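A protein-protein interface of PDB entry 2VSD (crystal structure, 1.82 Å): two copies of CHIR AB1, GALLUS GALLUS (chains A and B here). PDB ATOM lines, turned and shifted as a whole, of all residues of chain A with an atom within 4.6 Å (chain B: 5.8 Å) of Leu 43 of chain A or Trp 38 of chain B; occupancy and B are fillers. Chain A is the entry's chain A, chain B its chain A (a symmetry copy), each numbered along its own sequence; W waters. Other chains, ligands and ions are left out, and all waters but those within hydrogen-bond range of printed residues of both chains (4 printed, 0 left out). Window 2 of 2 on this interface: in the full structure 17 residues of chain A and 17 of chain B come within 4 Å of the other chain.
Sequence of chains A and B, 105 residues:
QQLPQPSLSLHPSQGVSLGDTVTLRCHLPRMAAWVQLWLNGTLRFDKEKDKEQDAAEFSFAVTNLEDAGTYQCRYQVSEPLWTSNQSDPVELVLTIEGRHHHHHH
The indole nitrogen (NE1) of Trp 38 of chain A sits at hydrogen-bond distance from the side-chain amide oxygen (OE1) of Gln 36 of chain A (2.9 Å). The side-chain amide oxygen (OE1) of Gln 36 of chain B sits at hydrogen-bond distance from the indole nitrogen (NE1) of Trp 38 of chain B. The backbone carbonyl oxygen (O) of Arg 74 of chain B is in hydrogen-bond range of the backbone NH (N) of Gln 36 of chain B (2.8 Å). The backbone NH (N) of Trp 38 of chain B is in hydrogen-bond range of the backbone carbonyl oxygen (O) of Gln 72 of chain B.
Printed residues of chain B within 4 Å of Gln 36 of chain A: Gln 36. Leu 37 of chain A touches none of the printed residues of chain B. Of the printed residues of chain B, Trp 38 of chain A touches Leu 43 (3.9 Å). Of the printed residues of chain B, Leu 43 of chain A touches Trp 38 and Leu 43. Of the printed residues of chain A, Gln 36 of chain B touches Gln 36 (3.6 Å). Of chain A, only Leu 43 (3.9 Å) comes within 4 Å of Trp 38 of chain B. Of the printed residues of chain A, Thr 42 of chain B touches Thr 42. Printed residues of chain A within 4 Å of Leu 43 of chain B: Trp 38 and Leu 43. The nearest printed residue of chain A that does not touch Trp 38 of chain B is Arg 44 of chain A (6.1 Å). The nearest printed residue of chain A that does not touch Thr 42 of chain B is Leu 43 of chain A (4.8 Å).
Water W3 bridges the backbone carbonyl oxygen (O) of Leu 43 of chain A (2.8 Å) and the backbone NH (N) of Leu 43 of chain B (3.0 Å). Water W1 bridges O of Leu 43 of chain B and N of Leu 43 of chain A. Water W2 lies within hydrogen-bond range of the side-chain amide nitrogen (NE2) of Gln 36 of chain A and the side-chain amide nitrogen (NE2) of Gln 36 of chain B. Water W4 bridges NE2 of Gln 36 of chain B (2.8 Å) and NE2 of Gln 36 of chain A (3.2 Å).
Gln 36 of chain B touches its own counterpart, Gln 36 of chain A. Trp 38 of chain A touches Leu 43 of chain B, and with the chains exchanged Leu 43 of chain A touches Trp 38 of chain B. Thr 42 of chain B touches its own counterpart, Thr 42 of chain A. Leu 43 of chain B touches its own counterpart, Leu 43 of chain A. Of the 5 pairs that touch across the chains among the printed residues, 5 have their exchanged pair printed and touching as well.
Hydrophobic or aromatic side chains of chain A within 4 Å of the printed part of chain B: Trp 38 and Leu 43. Hydrophobic or aromatic side chains of chain B that line the printed part of chain A: Trp 38 and Leu 43. Among the printed residues, no Asp or Glu carboxylate lies within 4 Å of a Lys or Arg side-chain nitrogen of the other chain.
Among the printed residues, pairs that only touch across the chains: Gln 36 of chain A with Gln 36 of chain B (3.6 Å), Trp 38 of chain A with Leu 43 of chain B (3.9 Å), Thr 42 of chain A with Thr 42 of chain B (3.4 Å), Leu 43 of chain A with Trp 38 of chain B (3.9 Å) and Leu 43 of chain A with Leu 43 of chain B (3.8 Å).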
ATOM      1  N   GLN A  36      -6.562  16.766   6.758  1.00  0.00           N
ATOM      2  CA  GLN A  36      -5.129  16.789   6.451  1.00  0.00           C
ATOM      3  C   GLN A  36      -4.614  15.415   6.030  1.00  0.00           C
ATOM      4  O   GLN A  36      -4.973  14.403   6.657  1.00  0.00           O
ATOM      5  CB  GLN A  36      -4.372  17.183   7.693  1.00  0.00           C
ATOM      6  CG  GLN A  36      -4.756  18.573   8.195  1.00  0.00           C
ATOM      7  CD  GLN A  36      -4.022  18.997   9.444  1.00  0.00           C
ATOM      8  OE1 GLN A  36      -3.492  18.172  10.203  1.00  0.00           O
ATOM      9  NE2 GLN A  36      -4.019  20.320   9.696  1.00  0.00           N
ATOM     10  N   LEU A  37      -3.723  15.386   5.044  1.00  0.00           N
ATOM     11  CA  LEU A  37      -3.022  14.161   4.730  1.00  0.00           C
ATOM     12  C   LEU A  37      -1.572  14.338   5.150  1.00  0.00           C
ATOM     13  O   LEU A  37      -0.910  15.268   4.682  1.00  0.00           O
ATOM     14  CB  LEU A  37      -3.097  13.829   3.228  1.00  0.00           C
ATOM     15  CG  LEU A  37      -2.479  12.461   2.838  1.00  0.00           C
ATOM     16  CD1 LEU A  37      -3.380  11.276   3.272  1.00  0.00           C
ATOM     17  CD2 LEU A  37      -2.274  12.434   1.334  1.00  0.00           C
ATOM     18  N   TRP A  38      -1.092  13.387   5.947  1.00  0.00           N
ATOM     19  CA  TRP A  38       0.252  13.410   6.532  1.00  0.00           C
ATOM     20  C   TRP A  38       1.040  12.269   5.936  1.00  0.00           C
ATOM     21  O   TRP A  38       0.487  11.163   5.722  1.00  0.00           O
ATOM     22  CB  TRP A  38       0.169  13.178   8.032  1.00  0.00           C
ATOM     23  CG  TRP A  38      -0.370  14.371   8.745  1.00  0.00           C
ATOM     24  CD1 TRP A  38      -1.637  14.882   8.648  1.00  0.00           C
ATOM     25  CD2 TRP A  38       0.350  15.215   9.647  1.00  0.00           C
ATOM     26  NE1 TRP A  38      -1.756  15.999   9.482  1.00  0.00           N
ATOM     27  CE2 TRP A  38      -0.549  16.225  10.089  1.00  0.00           C
ATOM     28  CE3 TRP A  38       1.665  15.203  10.149  1.00  0.00           C
ATOM     29  CZ2 TRP A  38      -0.169  17.241  10.982  1.00  0.00           C
ATOM     30  CZ3 TRP A  38       2.052  16.205  11.055  1.00  0.00           C
ATOM     31  CH2 TRP A  38       1.124  17.221  11.466  1.00  0.00           C
ATOM     32  N   GLY A  41       4.729  11.408   9.110  1.00  0.00           N
ATOM     33  CA  GLY A  41       4.615  12.256  10.310  1.00  0.00           C
ATOM     34  C   GLY A  41       4.757  13.747  10.036  1.00  0.00           C
ATOM     35  O   GLY A  41       4.939  14.542  10.980  1.00  0.00           O
ATOM     36  N   THR A  42       4.673  14.146   8.762  1.00  0.00           N
ATOM     37  CA  THR A  42       4.720  15.561   8.377  1.00  0.00           C
ATOM     38  C   THR A  42       3.518  15.833   7.458  1.00  0.00           C
ATOM     39  O   THR A  42       3.175  14.999   6.617  1.00  0.00           O
ATOM     40  CB  THR A  42       6.057  15.878   7.647  1.00  0.00           C
ATOM     41  OG1 THR A  42       7.159  15.719   8.564  1.00  0.00           O
ATOM     42  CG2 THR A  42       6.071  17.292   7.061  1.00  0.00           C
ATOM     43  N   LEU A  43       2.866  16.976   7.640  1.00  0.00           N
ATOM     44  CA  LEU A  43       1.712  17.340   6.796  1.00  0.00           C
ATOM     45  C   LEU A  43       2.114  17.448   5.330  1.00  0.00           C
ATOM     46  O   LEU A  43       3.115  18.159   5.003  1.00  0.00           O
ATOM     47  CB  LEU A  43       1.131  18.699   7.271  1.00  0.00           C
ATOM     48  CG  LEU A  43       0.015  19.273   6.399  1.00  0.00           C
ATOM     49  CD1 LEU A  43      -1.215  18.478   6.747  1.00  0.00           C
ATOM     50  CD2 LEU A  43      -0.251  20.802   6.633  1.00  0.00           C
ATOM     51  N   ARG A  44       1.348  16.754   4.457  1.00  0.00           N
ATOM     52  CA  ARG A  44       1.562  16.872   3.023  1.00  0.00           C
ATOM     53  C   ARG A  44       0.545  17.793   2.333  1.00  0.00           C
ATOM     54  O   ARG A  44       0.940  18.775   1.687  1.00  0.00           O
ATOM     55  CB  ARG A  44       1.631  15.490   2.332  1.00  0.00           C
ATOM     56  CG  ARG A  44       2.133  15.644   0.896  1.00  0.00           C
ATOM     57  CD  ARG A  44       2.319  14.363   0.170  1.00  0.00           C
ATOM     58  NE  ARG A  44       2.756  14.668  -1.198  1.00  0.00           N
ATOM     59  CZ  ARG A  44       3.073  13.777  -2.132  1.00  0.00           C
ATOM     60  NH1 ARG A  44       3.065  12.471  -1.862  1.00  0.00           N
ATOM     61  NH2 ARG A  44       3.435  14.210  -3.342  1.00  0.00           N
ATOM     62  N   PHE A  45      -0.745  17.483   2.480  1.00  0.00           N
ATOM     63  CA  PHE A  45      -1.836  18.239   1.850  1.00  0.00           C
ATOM     64  C   PHE A  45      -2.904  18.497   2.879  1.00  0.00           C
ATOM     65  O   PHE A  45      -3.041  17.764   3.876  1.00  0.00           O
ATOM     66  CB  PHE A  45      -2.519  17.414   0.752  1.00  0.00           C
ATOM     67  CG  PHE A  45      -1.610  17.003  -0.368  1.00  0.00           C
ATOM     68  CD1 PHE A  45      -0.949  17.966  -1.131  1.00  0.00           C
ATOM     69  CD2 PHE A  45      -1.461  15.661  -0.693  1.00  0.00           C
ATOM     70  CE1 PHE A  45      -0.145  17.598  -2.211  1.00  0.00           C
ATOM     71  CE2 PHE A  45      -0.655  15.278  -1.760  1.00  0.00           C
ATOM     72  CZ  PHE A  45       0.000  16.240  -2.510  1.00  0.00           C
ATOM     73  N   GLN B  36      -1.597  27.677  12.550  1.00  0.00           N
ATOM     74  CA  GLN B  36      -0.451  26.851  12.162  1.00  0.00           C
ATOM     75  C   GLN B  36       0.840  27.661  12.096  1.00  0.00           C
ATOM     76  O   GLN B  36       0.836  28.786  11.567  1.00  0.00           O
ATOM     77  CB  GLN B  36      -0.696  26.297  10.783  1.00  0.00           C
ATOM     78  CG  GLN B  36      -1.941  25.415  10.720  1.00  0.00           C
ATOM     79  CD  GLN B  36      -2.222  24.850   9.349  1.00  0.00           C
ATOM     80  OE1 GLN B  36      -1.757  25.364   8.321  1.00  0.00           O
ATOM     81  NE2 GLN B  36      -3.042  23.781   9.316  1.00  0.00           N
ATOM     82  N   LEU B  37       1.942  27.069  12.545  1.00  0.00           N
ATOM     83  CA  LEU B  37       3.238  27.671  12.321  1.00  0.00           C
ATOM     84  C   LEU B  37       3.979  26.810  11.310  1.00  0.00           C
ATOM     85  O   LEU B  37       4.168  25.615  11.549  1.00  0.00           O
ATOM     86  CB  LEU B  37       4.053  27.772  13.623  1.00  0.00           C
ATOM     87  CG  LEU B  37       5.401  28.527  13.484  1.00  0.00           C
ATOM     88  CD1 LEU B  37       5.193  30.057  13.348  1.00  0.00           C
ATOM     89  CD2 LEU B  37       6.254  28.224  14.702  1.00  0.00           C
ATOM     90  N   TRP B  38       4.458  27.462  10.254  1.00  0.00           N
ATOM     91  CA  TRP B  38       5.130  26.811   9.126  1.00  0.00           C
ATOM     92  C   TRP B  38       6.572  27.256   9.120  1.00  0.00           C
ATOM     93  O   TRP B  38       6.868  28.442   9.405  1.00  0.00           O
ATOM     94  CB  TRP B  38       4.503  27.264   7.817  1.00  0.00           C
ATOM     95  CG  TRP B  38       3.157  26.659   7.613  1.00  0.00           C
ATOM     96  CD1 TRP B  38       2.030  26.894   8.355  1.00  0.00           C
ATOM     97  CD2 TRP B  38       2.802  25.701   6.612  1.00  0.00           C
ATOM     98  NE1 TRP B  38       0.965  26.146   7.840  1.00  0.00           N
ATOM     99  CE2 TRP B  38       1.422  25.402   6.784  1.00  0.00           C
ATOM    100  CE3 TRP B  38       3.510  25.082   5.565  1.00  0.00           C
ATOM    101  CZ2 TRP B  38       0.738  24.481   5.974  1.00  0.00           C
ATOM    102  CZ3 TRP B  38       2.833  24.172   4.738  1.00  0.00           C
ATOM    103  CH2 TRP B  38       1.443  23.878   4.951  1.00  0.00           C
ATOM    104  N   LEU B  39       7.461  26.311   8.817  1.00  0.00           N
ATOM    105  CA  LEU B  39       8.906  26.591   8.718  1.00  0.00           C
ATOM    106  C   LEU B  39       9.396  26.128   7.345  1.00  0.00           C
ATOM    107  O   LEU B  39       9.216  24.939   7.002  1.00  0.00           O
ATOM    108  CB  LEU B  39       9.671  25.873   9.859  1.00  0.00           C
ATOM    109  CG  LEU B  39      11.206  25.823   9.737  1.00  0.00           C
ATOM    110  CD1 LEU B  39      11.804  27.259   9.570  1.00  0.00           C
ATOM    111  CD2 LEU B  39      11.864  25.131  10.936  1.00  0.00           C
ATOM    112  N   ASN B  40       9.972  27.049   6.549  1.00  0.00           N
ATOM    113  CA  ASN B  40      10.499  26.694   5.217  1.00  0.00           C
ATOM    114  C   ASN B  40       9.430  26.017   4.352  1.00  0.00           C
ATOM    115  O   ASN B  40       9.722  25.099   3.550  1.00  0.00           O
ATOM    116  CB  ASN B  40      11.727  25.772   5.316  1.00  0.00           C
ATOM    117  CG  ASN B  40      12.911  26.417   6.016  1.00  0.00           C
ATOM    118  OD1 ASN B  40      12.915  27.622   6.315  1.00  0.00           O
ATOM    119  ND2 ASN B  40      13.913  25.564   6.326  1.00  0.00           N
ATOM    120  N   GLY B  41       8.186  26.464   4.517  1.00  0.00           N
ATOM    121  CA  GLY B  41       7.100  25.990   3.641  1.00  0.00           C
ATOM    122  C   GLY B  41       6.532  24.632   4.030  1.00  0.00           C
ATOM    123  O   GLY B  41       5.803  24.007   3.233  1.00  0.00           O
ATOM    124  N   THR B  42       6.847  24.162   5.241  1.00  0.00           N
ATOM    125  CA  THR B  42       6.304  22.900   5.760  1.00  0.00           C
ATOM    126  C   THR B  42       5.730  23.183   7.158  1.00  0.00           C
ATOM    127  O   THR B  42       6.318  23.940   7.933  1.00  0.00           O
ATOM    128  CB  THR B  42       7.419  21.819   5.829  1.00  0.00           C
ATOM    129  OG1 THR B  42       7.863  21.496   4.495  1.00  0.00           O
ATOM    130  CG2 THR B  42       6.946  20.548   6.539  1.00  0.00           C
ATOM    131  N   LEU B  43       4.573  22.604   7.464  1.00  0.00           N
ATOM    132  CA  LEU B  43       3.949  22.794   8.787  1.00  0.00           C
ATOM    133  C   LEU B  43       4.853  22.279   9.901  1.00  0.00           C
ATOM    134  O   LEU B  43       5.335  21.106   9.829  1.00  0.00           O
ATOM    135  CB  LEU B  43       2.593  22.039   8.834  1.00  0.00           C
ATOM    136  CG  LEU B  43       1.898  22.030  10.194  1.00  0.00           C
ATOM    137  CD1 LEU B  43       1.288  23.398  10.342  1.00  0.00           C
ATOM    138  CD2 LEU B  43       0.786  20.931  10.331  1.00  0.00           C
ATOM    139  N   ARG B  44       5.081  23.140  10.919  1.00  0.00           N
ATOM    140  CA  ARG B  44       5.831  22.722  12.093  1.00  0.00           C
ATOM    141  C   ARG B  44       4.937  22.397  13.298  1.00  0.00           C
ATOM    142  O   ARG B  44       4.991  21.274  13.823  1.00  0.00           O
ATOM    143  CB  ARG B  44       6.935  23.738  12.468  1.00  0.00           C
ATOM    144  CG  ARG B  44       7.872  23.136  13.516  1.00  0.00           C
ATOM    145  CD  ARG B  44       9.021  24.000  13.882  1.00  0.00           C
ATOM    146  NE  ARG B  44       9.799  23.316  14.923  1.00  0.00           N
ATOM    147  CZ  ARG B  44      10.929  23.755  15.466  1.00  0.00           C
ATOM    148  NH1 ARG B  44      11.496  24.888  15.045  1.00  0.00           N
ATOM    149  NH2 ARG B  44      11.513  23.027  16.421  1.00  0.00           N
ATOM    150  N   PHE B  45       4.120  23.365  13.720  1.00  0.00           N
ATOM    151  CA  PHE B  45       3.232  23.225  14.883  1.00  0.00           C
ATOM    152  C   PHE B  45       1.863  23.727  14.511  1.00  0.00           C
ATOM    153  O   PHE B  45       1.696  24.555  13.595  1.00  0.00           O
ATOM    154  CB  PHE B  45       3.693  24.119  16.040  1.00  0.00           C
ATOM    155  CG  PHE B  45       5.074  23.817  16.544  1.00  0.00           C
ATOM    156  CD1 PHE B  45       5.381  22.551  17.045  1.00  0.00           C
ATOM    157  CD2 PHE B  45       6.045  24.809  16.566  1.00  0.00           C
ATOM    158  CE1 PHE B  45       6.645  22.274  17.568  1.00  0.00           C
ATOM    159  CE2 PHE B  45       7.312  24.545  17.074  1.00  0.00           C
ATOM    160  CZ  PHE B  45       7.610  23.286  17.567  1.00  0.00           C
ATOM    161  N   THR B  70      12.717  30.232   7.584  1.00  0.00           N
ATOM    162  CA  THR B  70      11.625  31.163   7.292  1.00  0.00           C
ATOM    163  C   THR B  70      10.331  30.706   7.943  1.00  0.00           C
ATOM    164  O   THR B  70       9.776  29.657   7.569  1.00  0.00           O
ATOM    165  CB  THR B  70      11.411  31.304   5.796  1.00  0.00           C
ATOM    166  OG1 THR B  70      12.657  31.605   5.188  1.00  0.00           O
ATOM    167  CG2 THR B  70      10.395  32.459   5.514  1.00  0.00           C
ATOM    168  N   TYR B  71       9.893  31.465   8.941  1.00  0.00           N
ATOM    169  CA  TYR B  71       8.642  31.183   9.651  1.00  0.00           C
ATOM    170  C   TYR B  71       7.451  31.967   9.109  1.00  0.00           C
ATOM    171  O   TYR B  71       7.559  33.155   8.805  1.00  0.00           O
ATOM    172  CB  TYR B  71       8.781  31.430  11.147  1.00  0.00           C
ATOM    173  CG  TYR B  71       9.620  30.365  11.835  1.00  0.00           C
ATOM    174  CD1 TYR B  71      11.024  30.486  11.892  1.00  0.00           C
ATOM    175  CD2 TYR B  71       9.020  29.238  12.398  1.00  0.00           C
ATOM    176  CE1 TYR B  71      11.808  29.520  12.528  1.00  0.00           C
ATOM    177  CE2 TYR B  71       9.816  28.235  13.024  1.00  0.00           C
ATOM    178  CZ  TYR B  71      11.193  28.404  13.077  1.00  0.00           C
ATOM    179  OH  TYR B  71      11.974  27.433  13.674  1.00  0.00           O
ATOM    180  N   GLN B  72       6.315  31.288   9.015  1.00  0.00           N
ATOM    181  CA  GLN B  72       5.056  31.919   8.611  1.00  0.00           C
ATOM    182  C   GLN B  72       3.931  31.343   9.416  1.00  0.00           C
ATOM    183  O   GLN B  72       4.058  30.226   9.942  1.00  0.00           O
ATOM    184  CB  GLN B  72       4.784  31.660   7.135  1.00  0.00           C
ATOM    185  CG  GLN B  72       5.691  32.413   6.205  1.00  0.00           C
ATOM    186  CD  GLN B  72       5.572  31.908   4.794  1.00  0.00           C
ATOM    187  OE1 GLN B  72       5.955  30.779   4.498  1.00  0.00           O
ATOM    188  NE2 GLN B  72       4.997  32.725   3.915  1.00  0.00           N
ATOM    189  N   CYS B  73       2.805  32.057   9.489  1.00  0.00           N
ATOM    190  CA  CYS B  73       1.627  31.471  10.133  1.00  0.00           C
ATOM    191  C   CYS B  73       0.383  31.607   9.250  1.00  0.00           C
ATOM    192  O   CYS B  73       0.343  32.478   8.367  1.00  0.00           O
ATOM    193  CB  CYS B  73       1.420  31.994  11.576  1.00  0.00           C
ATOM    194  SG  CYS B  73       0.903  33.733  11.743  1.00  0.00           S
ATOM    195  N   ARG B  74      -0.576  30.703   9.484  1.00  0.00           N
ATOM    196  CA  ARG B  74      -1.777  30.513   8.677  1.00  0.00           C
ATOM    197  C   ARG B  74      -2.855  30.166   9.692  1.00  0.00           C
ATOM    198  O   ARG B  74      -2.570  29.510  10.701  1.00  0.00           O
ATOM    199  CB  ARG B  74      -1.512  29.296   7.782  1.00  0.00           C
ATOM    200  CG  ARG B  74      -2.528  28.910   6.796  1.00  0.00           C
ATOM    201  CD  ARG B  74      -1.878  27.889   5.924  1.00  0.00           C
ATOM    202  NE  ARG B  74      -2.761  27.353   4.904  1.00  0.00           N
ATOM    203  CZ  ARG B  74      -3.180  26.100   4.834  1.00  0.00           C
ATOM    204  NH1 ARG B  74      -2.850  25.192   5.753  1.00  0.00           N
ATOM    205  NH2 ARG B  74      -3.985  25.768   3.838  1.00  0.00           N
ATOM    206  N   GLN B  86      -0.788  32.532   4.046  1.00  0.00           N
ATOM    207  CA  GLN B  86       0.379  32.663   4.940  1.00  0.00           C
ATOM    208  C   GLN B  86       0.632  34.115   5.309  1.00  0.00           C
ATOM    209  O   GLN B  86       0.495  35.006   4.463  1.00  0.00           O
ATOM    210  CB  GLN B  86       1.621  32.133   4.260  1.00  0.00           C
ATOM    211  CG  GLN B  86       1.685  30.604   4.055  1.00  0.00           C
ATOM    212  CD  GLN B  86       1.705  29.817   5.341  1.00  0.00           C
ATOM    213  OE1 GLN B  86       1.786  30.381   6.441  1.00  0.00           O
ATOM    214  NE2 GLN B  86       1.602  28.494   5.214  1.00  0.00           N
HETATM  215  O   HOH W   1       3.989  18.703   9.803  1.00  0.00           O
HETATM  216  O   HOH W   2      -5.226  22.063   7.814  1.00  0.00           O
HETATM  217  O   HOH W   3       3.453  20.876   5.299  1.00  0.00           O
HETATM  218  O   HOH W   4      -3.960  22.702  11.772  1.00  0.00           O
